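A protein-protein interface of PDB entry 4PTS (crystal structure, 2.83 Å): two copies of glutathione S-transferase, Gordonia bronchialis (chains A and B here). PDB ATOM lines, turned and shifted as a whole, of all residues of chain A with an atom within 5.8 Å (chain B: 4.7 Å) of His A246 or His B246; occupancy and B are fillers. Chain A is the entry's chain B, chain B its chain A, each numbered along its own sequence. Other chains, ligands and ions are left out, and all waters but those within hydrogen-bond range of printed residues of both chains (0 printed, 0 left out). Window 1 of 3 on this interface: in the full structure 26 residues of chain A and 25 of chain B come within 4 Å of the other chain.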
ATOM      1  N   ARG A 240      22.490 -13.809 -15.356  1.00  0.00           N
ATOM      2  CA  ARG A 240      21.359 -13.247 -16.073  1.00  0.00           C
ATOM      3  C   ARG A 240      21.200 -13.772 -17.481  1.00  0.00           C
ATOM      4  O   ARG A 240      20.224 -13.454 -18.153  1.00  0.00           O
ATOM      5  CB  ARG A 240      21.504 -11.735 -16.107  1.00  0.00           C
ATOM      6  CG  ARG A 240      21.122 -11.105 -14.790  1.00  0.00           C
ATOM      7  CD  ARG A 240      21.736  -9.727 -14.641  1.00  0.00           C
ATOM      8  NE  ARG A 240      21.302  -9.167 -13.386  1.00  0.00           N
ATOM      9  CZ  ARG A 240      21.767  -9.530 -12.205  1.00  0.00           C
ATOM     10  NH1 ARG A 240      22.735 -10.432 -12.081  1.00  0.00           N
ATOM     11  NH2 ARG A 240      21.240  -8.962 -11.141  1.00  0.00           N
ATOM     12  N   PHE A 241      22.129 -14.611 -17.897  1.00  0.00           N
ATOM     13  CA  PHE A 241      22.200 -15.004 -19.273  1.00  0.00           C
ATOM     14  C   PHE A 241      20.967 -15.752 -19.727  1.00  0.00           C
ATOM     15  O   PHE A 241      20.220 -15.257 -20.575  1.00  0.00           O
ATOM     16  CB  PHE A 241      23.428 -15.842 -19.540  1.00  0.00           C
ATOM     17  CG  PHE A 241      23.773 -15.904 -20.975  1.00  0.00           C
ATOM     18  CD1 PHE A 241      24.555 -14.921 -21.549  1.00  0.00           C
ATOM     19  CD2 PHE A 241      23.268 -16.903 -21.773  1.00  0.00           C
ATOM     20  CE1 PHE A 241      24.864 -14.956 -22.903  1.00  0.00           C
ATOM     21  CE2 PHE A 241      23.565 -16.947 -23.131  1.00  0.00           C
ATOM     22  CZ  PHE A 241      24.370 -15.972 -23.698  1.00  0.00           C
ATOM     23  N   ASP A 242      20.743 -16.933 -19.168  1.00  0.00           N
ATOM     24  CA  ASP A 242      19.571 -17.731 -19.570  1.00  0.00           C
ATOM     25  C   ASP A 242      18.223 -17.064 -19.204  1.00  0.00           C
ATOM     26  O   ASP A 242      17.242 -17.167 -19.938  1.00  0.00           O
ATOM     27  CB  ASP A 242      19.652 -19.148 -18.972  1.00  0.00           C
ATOM     28  CG  ASP A 242      20.648 -20.041 -19.706  1.00  0.00           C
ATOM     29  OD1 ASP A 242      21.297 -19.559 -20.676  1.00  0.00           O
ATOM     30  OD2 ASP A 242      20.760 -21.241 -19.327  1.00  0.00           O
ATOM     31  N   ALA A 243      18.180 -16.388 -18.065  1.00  0.00           N
ATOM     32  CA  ALA A 243      16.942 -15.798 -17.610  1.00  0.00           C
ATOM     33  C   ALA A 243      16.541 -14.614 -18.479  1.00  0.00           C
ATOM     34  O   ALA A 243      15.358 -14.379 -18.675  1.00  0.00           O
ATOM     35  CB  ALA A 243      17.071 -15.384 -16.157  1.00  0.00           C
ATOM     36  N   VAL A 244      17.513 -13.891 -19.024  1.00  0.00           N
ATOM     37  CA  VAL A 244      17.193 -12.680 -19.754  1.00  0.00           C
ATOM     38  C   VAL A 244      17.908 -12.533 -21.071  1.00  0.00           C
ATOM     39  O   VAL A 244      17.278 -12.423 -22.119  1.00  0.00           O
ATOM     40  CB  VAL A 244      17.547 -11.432 -18.940  1.00  0.00           C
ATOM     41  CG1 VAL A 244      17.048 -10.195 -19.646  1.00  0.00           C
ATOM     42  CG2 VAL A 244      16.939 -11.526 -17.559  1.00  0.00           C
ATOM     43  N   TYR A 245      19.223 -12.488 -21.020  1.00  0.00           N
ATOM     44  CA  TYR A 245      19.985 -12.060 -22.165  1.00  0.00           C
ATOM     45  C   TYR A 245      19.764 -12.938 -23.401  1.00  0.00           C
ATOM     46  O   TYR A 245      19.633 -12.471 -24.526  1.00  0.00           O
ATOM     47  CB  TYR A 245      21.454 -12.010 -21.771  1.00  0.00           C
ATOM     48  CG  TYR A 245      21.772 -11.045 -20.630  1.00  0.00           C
ATOM     49  CD1 TYR A 245      21.051  -9.851 -20.466  1.00  0.00           C
ATOM     50  CD2 TYR A 245      22.819 -11.300 -19.751  1.00  0.00           C
ATOM     51  CE1 TYR A 245      21.344  -8.963 -19.445  1.00  0.00           C
ATOM     52  CE2 TYR A 245      23.125 -10.416 -18.732  1.00  0.00           C
ATOM     53  CZ  TYR A 245      22.382  -9.247 -18.571  1.00  0.00           C
ATOM     54  OH  TYR A 245      22.676  -8.330 -17.570  1.00  0.00           O
ATOM     55  N   HIS A 246      19.685 -14.224 -23.161  1.00  0.00           N
ATOM     56  CA  HIS A 246      19.451 -15.180 -24.220  1.00  0.00           C
ATOM     57  C   HIS A 246      18.187 -14.925 -25.075  1.00  0.00           C
ATOM     58  O   HIS A 246      18.236 -14.997 -26.304  1.00  0.00           O
ATOM     59  CB  HIS A 246      19.377 -16.574 -23.615  1.00  0.00           C
ATOM     60  CG  HIS A 246      19.198 -17.625 -24.637  1.00  0.00           C
ATOM     61  ND1 HIS A 246      17.968 -18.139 -24.961  1.00  0.00           N
ATOM     62  CD2 HIS A 246      20.086 -18.212 -25.461  1.00  0.00           C
ATOM     63  CE1 HIS A 246      18.112 -19.032 -25.920  1.00  0.00           C
ATOM     64  NE2 HIS A 246      19.388 -19.089 -26.245  1.00  0.00           N
ATOM     65  N   GLY A 247      17.052 -14.702 -24.423  1.00  0.00           N
ATOM     66  CA  GLY A 247      15.818 -14.405 -25.127  1.00  0.00           C
ATOM     67  C   GLY A 247      15.665 -12.908 -25.318  1.00  0.00           C
ATOM     68  O   GLY A 247      15.751 -12.378 -26.421  1.00  0.00           O
ATOM     69  N   HIS A 248      15.427 -12.209 -24.225  1.00  0.00           N
ATOM     70  CA  HIS A 248      15.197 -10.779 -24.283  1.00  0.00           C
ATOM     71  C   HIS A 248      16.146 -10.008 -25.205  1.00  0.00           C
ATOM     72  O   HIS A 248      15.707  -9.230 -26.058  1.00  0.00           O
ATOM     73  CB  HIS A 248      15.291 -10.223 -22.876  1.00  0.00           C
ATOM     74  CG  HIS A 248      14.767  -8.835 -22.755  1.00  0.00           C
ATOM     75  ND1 HIS A 248      13.544  -8.461 -23.270  1.00  0.00           N
ATOM     76  CD2 HIS A 248      15.293  -7.732 -22.177  1.00  0.00           C
ATOM     77  CE1 HIS A 248      13.347  -7.180 -23.022  1.00  0.00           C
ATOM     78  NE2 HIS A 248      14.387  -6.719 -22.353  1.00  0.00           N
ATOM     79  N   PHE A 249      17.442 -10.229 -25.020  1.00  0.00           N
ATOM     80  CA  PHE A 249      18.473  -9.533 -25.792  1.00  0.00           C
ATOM     81  C   PHE A 249      18.943 -10.328 -27.001  1.00  0.00           C
ATOM     82  O   PHE A 249      19.862  -9.914 -27.701  1.00  0.00           O
ATOM     83  CB  PHE A 249      19.678  -9.212 -24.912  1.00  0.00           C
ATOM     84  CG  PHE A 249      19.463  -8.083 -23.947  1.00  0.00           C
ATOM     85  CD1 PHE A 249      18.300  -7.315 -23.951  1.00  0.00           C
ATOM     86  CD2 PHE A 249      20.469  -7.747 -23.067  1.00  0.00           C
ATOM     87  CE1 PHE A 249      18.144  -6.259 -23.079  1.00  0.00           C
ATOM     88  CE2 PHE A 249      20.318  -6.697 -22.193  1.00  0.00           C
ATOM     89  CZ  PHE A 249      19.151  -5.951 -22.192  1.00  0.00           C
ATOM     90  N   LYS A 250      18.332 -11.488 -27.223  1.00  0.00           N
ATOM     91  CA  LYS A 250      18.628 -12.310 -28.398  1.00  0.00           C
ATOM     92  C   LYS A 250      20.086 -12.759 -28.507  1.00  0.00           C
ATOM     93  O   LYS A 250      20.591 -12.949 -29.603  1.00  0.00           O
ATOM     94  CB  LYS A 250      18.246 -11.563 -29.658  1.00  0.00           C
ATOM     95  CG  LYS A 250      16.779 -11.237 -29.742  1.00  0.00           C
ATOM     96  CD  LYS A 250      16.492 -10.473 -31.013  1.00  0.00           C
ATOM     97  CE  LYS A 250      15.022 -10.193 -31.189  1.00  0.00           C
ATOM     98  NZ  LYS A 250      14.684  -8.903 -30.527  1.00  0.00           N
ATOM     99  N   CYS A 251      20.739 -12.964 -27.367  1.00  0.00           N
ATOM    100  CA  CYS A 251      22.099 -13.480 -27.340  1.00  0.00           C
ATOM    101  C   CYS A 251      22.056 -14.991 -27.416  1.00  0.00           C
ATOM    102  O   CYS A 251      22.391 -15.662 -26.445  1.00  0.00           O
ATOM    103  CB  CYS A 251      22.783 -13.061 -26.050  1.00  0.00           C
ATOM    104  SG  CYS A 251      22.940 -11.276 -25.921  1.00  0.00           S
ATOM    105  N   ASN A 252      21.677 -15.529 -28.575  1.00  0.00           N
ATOM    106  CA  ASN A 252      21.135 -16.885 -28.593  1.00  0.00           C
ATOM    107  C   ASN A 252      21.859 -17.954 -29.400  1.00  0.00           C
ATOM    108  O   ASN A 252      21.207 -18.923 -29.824  1.00  0.00           O
ATOM    109  CB  ASN A 252      19.684 -16.833 -29.051  1.00  0.00           C
ATOM    110  CG  ASN A 252      19.568 -16.586 -30.518  1.00  0.00           C
ATOM    111  OD1 ASN A 252      20.450 -16.027 -31.135  1.00  0.00           O
ATOM    112  ND2 ASN A 252      18.478 -17.001 -31.080  1.00  0.00           N
ATOM    113  N   ARG A 253      23.179 -17.836 -29.560  1.00  0.00           N
ATOM    114  CA  ARG A 253      23.935 -18.934 -30.154  1.00  0.00           C
ATOM    115  C   ARG A 253      23.613 -20.244 -29.443  1.00  0.00           C
ATOM    116  O   ARG A 253      23.503 -21.309 -30.055  1.00  0.00           O
ATOM    117  CB  ARG A 253      25.442 -18.713 -30.074  1.00  0.00           C
ATOM    118  CG  ARG A 253      26.200 -19.613 -31.034  1.00  0.00           C
ATOM    119  CD  ARG A 253      27.693 -19.372 -31.036  1.00  0.00           C
ATOM    120  NE  ARG A 253      28.320 -19.969 -29.860  1.00  0.00           N
ATOM    121  CZ  ARG A 253      29.606 -19.840 -29.547  1.00  0.00           C
ATOM    122  NH1 ARG A 253      30.430 -19.140 -30.312  1.00  0.00           N
ATOM    123  NH2 ARG A 253      30.074 -20.409 -28.456  1.00  0.00           N
ATOM    124  N   SER A 254      23.433 -20.137 -28.135  1.00  0.00           N
ATOM    125  CA  SER A 254      23.273 -21.286 -27.294  1.00  0.00           C
ATOM    126  C   SER A 254      22.998 -20.762 -25.900  1.00  0.00           C
ATOM    127  O   SER A 254      23.412 -19.656 -25.564  1.00  0.00           O
ATOM    128  CB  SER A 254      24.567 -22.109 -27.346  1.00  0.00           C
ATOM    129  OG  SER A 254      24.966 -22.615 -26.067  1.00  0.00           O
ATOM    130  N   LYS A 255      22.290 -21.548 -25.099  1.00  0.00           N
ATOM    131  CA  LYS A 255      22.138 -21.224 -23.688  1.00  0.00           C
ATOM    132  C   LYS A 255      23.422 -21.450 -22.889  1.00  0.00           C
ATOM    133  O   LYS A 255      24.302 -22.253 -23.265  1.00  0.00           O
ATOM    134  CB  LYS A 255      21.026 -22.054 -23.046  1.00  0.00           C
ATOM    135  CG  LYS A 255      19.630 -21.531 -23.321  1.00  0.00           C
ATOM    136  CD  LYS A 255      18.564 -22.321 -22.526  1.00  0.00           C
ATOM    137  CE  LYS A 255      17.990 -21.647 -21.298  1.00  0.00           C
ATOM    138  NZ  LYS A 255      16.718 -22.342 -20.957  1.00  0.00           N
ATOM    139  N   LEU A 256      23.483 -20.779 -21.741  1.00  0.00           N
ATOM    140  CA  LEU A 256      24.586 -20.963 -20.833  1.00  0.00           C
ATOM    141  C   LEU A 256      24.703 -22.417 -20.447  1.00  0.00           C
ATOM    142  O   LEU A 256      25.777 -22.964 -20.521  1.00  0.00           O
ATOM    143  CB  LEU A 256      24.431 -20.142 -19.580  1.00  0.00           C
ATOM    144  CG  LEU A 256      25.638 -20.295 -18.663  1.00  0.00           C
ATOM    145  CD1 LEU A 256      26.946 -20.025 -19.399  1.00  0.00           C
ATOM    146  CD2 LEU A 256      25.502 -19.362 -17.468  1.00  0.00           C
ATOM    147  N   PHE B 241      11.018 -24.844 -32.748  1.00  0.00           N
ATOM    148  CA  PHE B 241      11.013 -24.564 -31.331  1.00  0.00           C
ATOM    149  C   PHE B 241      12.172 -23.700 -30.914  1.00  0.00           C
ATOM    150  O   PHE B 241      11.952 -22.564 -30.485  1.00  0.00           O
ATOM    151  CB  PHE B 241      11.026 -25.847 -30.517  1.00  0.00           C
ATOM    152  CG  PHE B 241      10.588 -25.637 -29.116  1.00  0.00           C
ATOM    153  CD1 PHE B 241       9.240 -25.660 -28.800  1.00  0.00           C
ATOM    154  CD2 PHE B 241      11.518 -25.367 -28.120  1.00  0.00           C
ATOM    155  CE1 PHE B 241       8.825 -25.438 -27.492  1.00  0.00           C
ATOM    156  CE2 PHE B 241      11.118 -25.142 -26.822  1.00  0.00           C
ATOM    157  CZ  PHE B 241       9.770 -25.172 -26.500  1.00  0.00           C
ATOM    158  N   ASP B 242      13.397 -24.219 -31.035  1.00  0.00           N
ATOM    159  CA  ASP B 242      14.589 -23.441 -30.634  1.00  0.00           C
ATOM    160  C   ASP B 242      14.821 -22.187 -31.495  1.00  0.00           C
ATOM    161  O   ASP B 242      15.213 -21.134 -30.997  1.00  0.00           O
ATOM    162  CB  ASP B 242      15.829 -24.321 -30.636  1.00  0.00           C
ATOM    163  CG  ASP B 242      15.890 -25.262 -29.421  1.00  0.00           C
ATOM    164  OD1 ASP B 242      14.970 -25.246 -28.573  1.00  0.00           O
ATOM    165  OD2 ASP B 242      16.885 -26.016 -29.312  1.00  0.00           O
ATOM    166  N   VAL B 244      12.564 -20.280 -32.944  1.00  0.00           N
ATOM    167  CA  VAL B 244      11.560 -19.225 -32.797  1.00  0.00           C
ATOM    168  C   VAL B 244      10.771 -19.268 -31.501  1.00  0.00           C
ATOM    169  O   VAL B 244      10.793 -18.334 -30.723  1.00  0.00           O
ATOM    170  CB  VAL B 244      10.521 -19.295 -33.912  1.00  0.00           C
ATOM    171  CG1 VAL B 244       9.599 -18.092 -33.819  1.00  0.00           C
ATOM    172  CG2 VAL B 244      11.206 -19.331 -35.252  1.00  0.00           C
ATOM    173  N   TYR B 245      10.063 -20.357 -31.289  1.00  0.00           N
ATOM    174  CA  TYR B 245       9.076 -20.401 -30.252  1.00  0.00           C
ATOM    175  C   TYR B 245       9.686 -20.153 -28.871  1.00  0.00           C
ATOM    176  O   TYR B 245       9.127 -19.446 -28.042  1.00  0.00           O
ATOM    177  CB  TYR B 245       8.362 -21.753 -30.321  1.00  0.00           C
ATOM    178  CG  TYR B 245       7.627 -22.032 -31.632  1.00  0.00           C
ATOM    179  CD1 TYR B 245       7.066 -21.000 -32.379  1.00  0.00           C
ATOM    180  CD2 TYR B 245       7.462 -23.331 -32.091  1.00  0.00           C
ATOM    181  CE1 TYR B 245       6.380 -21.249 -33.542  1.00  0.00           C
ATOM    182  CE2 TYR B 245       6.773 -23.593 -33.268  1.00  0.00           C
ATOM    183  CZ  TYR B 245       6.233 -22.545 -33.993  1.00  0.00           C
ATOM    184  OH  TYR B 245       5.550 -22.786 -35.179  1.00  0.00           O
ATOM    185  N   HIS B 246      10.854 -20.734 -28.636  1.00  0.00           N
ATOM    186  CA  HIS B 246      11.574 -20.584 -27.370  1.00  0.00           C
ATOM    187  C   HIS B 246      11.870 -19.128 -26.963  1.00  0.00           C
ATOM    188  O   HIS B 246      11.635 -18.739 -25.815  1.00  0.00           O
ATOM    189  CB  HIS B 246      12.888 -21.357 -27.430  1.00  0.00           C
ATOM    190  CG  HIS B 246      13.653 -21.301 -26.155  1.00  0.00           C
ATOM    191  ND1 HIS B 246      14.641 -20.372 -25.932  1.00  0.00           N
ATOM    192  CD2 HIS B 246      13.511 -21.994 -25.003  1.00  0.00           C
ATOM    193  CE1 HIS B 246      15.099 -20.518 -24.701  1.00  0.00           C
ATOM    194  NE2 HIS B 246      14.432 -21.498 -24.119  1.00  0.00           N
ATOM    195  N   GLY B 247      12.381 -18.327 -27.899  1.00  0.00           N
ATOM    196  CA  GLY B 247      12.636 -16.903 -27.642  1.00  0.00           C
ATOM    197  C   GLY B 247      11.464 -16.008 -28.013  1.00  0.00           C
ATOM    198  O   GLY B 247      10.766 -15.469 -27.176  1.00  0.00           O
ATOM    199  N   HIS B 248      11.215 -15.894 -29.296  1.00  0.00           N
ATOM    200  CA  HIS B 248      10.115 -15.088 -29.785  1.00  0.00           C
ATOM    201  C   HIS B 248       8.782 -15.231 -29.016  1.00  0.00           C
ATOM    202  O   HIS B 248       8.187 -14.229 -28.625  1.00  0.00           O
ATOM    203  CB  HIS B 248       9.878 -15.448 -31.248  1.00  0.00           C
ATOM    204  CG  HIS B 248       9.025 -14.463 -31.963  1.00  0.00           C
ATOM    205  ND1 HIS B 248       9.247 -13.103 -31.877  1.00  0.00           N
ATOM    206  CD2 HIS B 248       7.945 -14.631 -32.757  1.00  0.00           C
ATOM    207  CE1 HIS B 248       8.343 -12.479 -32.602  1.00  0.00           C
ATOM    208  NE2 HIS B 248       7.540 -13.380 -33.142  1.00  0.00           N
ATOM    209  N   LYS B 250       8.464 -16.998 -26.253  1.00  0.00           N
ATOM    210  CA  LYS B 250       8.750 -17.156 -24.820  1.00  0.00           C
ATOM    211  C   LYS B 250       8.353 -18.508 -24.242  1.00  0.00           C
ATOM    212  O   LYS B 250       8.009 -18.599 -23.077  1.00  0.00           O
ATOM    213  CB  LYS B 250       8.075 -16.051 -24.021  1.00  0.00           C
ATOM    214  CG  LYS B 250       8.572 -14.667 -24.373  1.00  0.00           C
ATOM    215  CD  LYS B 250       7.827 -13.609 -23.578  1.00  0.00           C
ATOM    216  CE  LYS B 250       8.380 -12.206 -23.791  1.00  0.00           C
ATOM    217  NZ  LYS B 250       7.723 -11.562 -24.951  1.00  0.00           N
ATOM    218  N   CYS B 251       8.407 -19.556 -25.054  1.00  0.00           N
ATOM    219  CA  CYS B 251       8.116 -20.902 -24.589  1.00  0.00           C
ATOM    220  C   CYS B 251       9.362 -21.487 -23.986  1.00  0.00           C
ATOM    221  O   CYS B 251       9.951 -22.410 -24.555  1.00  0.00           O
ATOM    222  CB  CYS B 251       7.679 -21.750 -25.768  1.00  0.00           C
ATOM    223  SG  CYS B 251       6.147 -21.148 -26.480  1.00  0.00           S
ATOM    224  N   ASN B 252       9.775 -20.971 -22.835  1.00  0.00           N
ATOM    225  CA  ASN B 252      11.186 -21.110 -22.452  1.00  0.00           C
ATOM    226  C   ASN B 252      11.530 -21.892 -21.184  1.00  0.00           C
ATOM    227  O   ASN B 252      12.549 -21.618 -20.559  1.00  0.00           O
ATOM    228  CB  ASN B 252      11.807 -19.731 -22.363  1.00  0.00           C
ATOM    229  CG  ASN B 252      11.357 -18.996 -21.142  1.00  0.00           C
ATOM    230  OD1 ASN B 252      10.273 -19.245 -20.628  1.00  0.00           O
ATOM    231  ND2 ASN B 252      12.179 -18.097 -20.659  1.00  0.00           N
ATOM    232  N   SER B 254      12.785 -24.531 -21.187  1.00  0.00           N
ATOM    233  CA  SER B 254      13.988 -25.207 -21.549  1.00  0.00           C
ATOM    234  C   SER B 254      13.982 -25.270 -23.066  1.00  0.00           C
ATOM    235  O   SER B 254      12.926 -25.257 -23.680  1.00  0.00           O
ATOM    236  CB  SER B 254      13.972 -26.615 -20.922  1.00  0.00           C
ATOM    237  OG  SER B 254      14.455 -27.613 -21.806  1.00  0.00           O
ATOM    238  N   LYS B 255      15.163 -25.312 -23.657  1.00  0.00           N
ATOM    239  CA  LYS B 255      15.286 -25.552 -25.078  1.00  0.00           C
ATOM    240  C   LYS B 255      15.008 -27.006 -25.448  1.00  0.00           C
ATOM    241  O   LYS B 255      15.112 -27.930 -24.611  1.00  0.00           O
ATOM    242  CB  LYS B 255      16.677 -25.200 -25.584  1.00  0.00           C
ATOM    243  CG  LYS B 255      16.848 -23.733 -25.847  1.00  0.00           C
ATOM    244  CD  LYS B 255      17.858 -23.426 -26.939  1.00  0.00           C
ATOM    245  CE  LYS B 255      19.218 -24.038 -26.765  1.00  0.00           C
ATOM    246  NZ  LYS B 255      19.976 -23.764 -28.015  1.00  0.00           N
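Ala A243 touches none of the printed residues of chain B.
Phe A249 touches none of the printed residues of chain B.
Of the printed residues of chain B, Lys A255 touches His B246 (3.99 Å) and Lys B255 (3.996 Å).
Of the printed residues of chain A, His B246 touches His A246 (3.6 Å) and Lys A255 (3.99 Å).
Of the printed residues of chain A, Lys B255 touches Lys A255.
The nearest residue of chain B that does not touch His A246 is Lys B255 (4.5 Å).
The nearest printed residue of chain A that does not touch Lys B255 is Ser A254 (4.2 Å).
His A246 touches its own counterpart, His B246.
Lys A255 touches His B246, but with the chains exchanged His A246 does not touch Lys B255 (4.5 Å).
Lys A255 touches its own counterpart, Lys B255.
Positions printed for both chains: 241, 242, 244, 245, 246, 247, 248, 250, 251, 252, 254 and 255.
Of the 3 pairs that touch across the chains among the printed residues, 2 have their exchanged pair printed and touching as well.
Among the printed residues, merely in contact across the chains: His A246 with His B246, Lys A255 with His B246 and Lys A255 with Lys B255.
Of the 12 printed residues of chain B, 2 touch a printed residue of chain A.
Hydrophobic or aromatic side chains of chain B within 4 Å of the printed part of chain A: His B246.
Of the 17 printed residues of chain A, 2 touch a printed residue of chain B.
Hydrophobic or aromatic side chains of chain A within 4 Å of the printed part of chain B: His A246.
Among the printed residues, 3 pairs touch across the chains.
The backbone carbonyl oxygen (O) of His A246 is in hydrogen-bond range of the backbone NH (N) of Cys A251, at 3.4 Å.
O of His B246 lies within hydrogen-bond range of N of Cys B251 (3.4 Å).
The backbone carbonyl oxygen (O) of Phe A241 sits at hydrogen-bond distance from the backbone NH (N) of His A246, 2.8 Å away.
The backbone NH (N) of His B246 lies within hydrogen-bond range of the backbone carbonyl oxygen (O) of Phe B241, at 2.8 Å.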
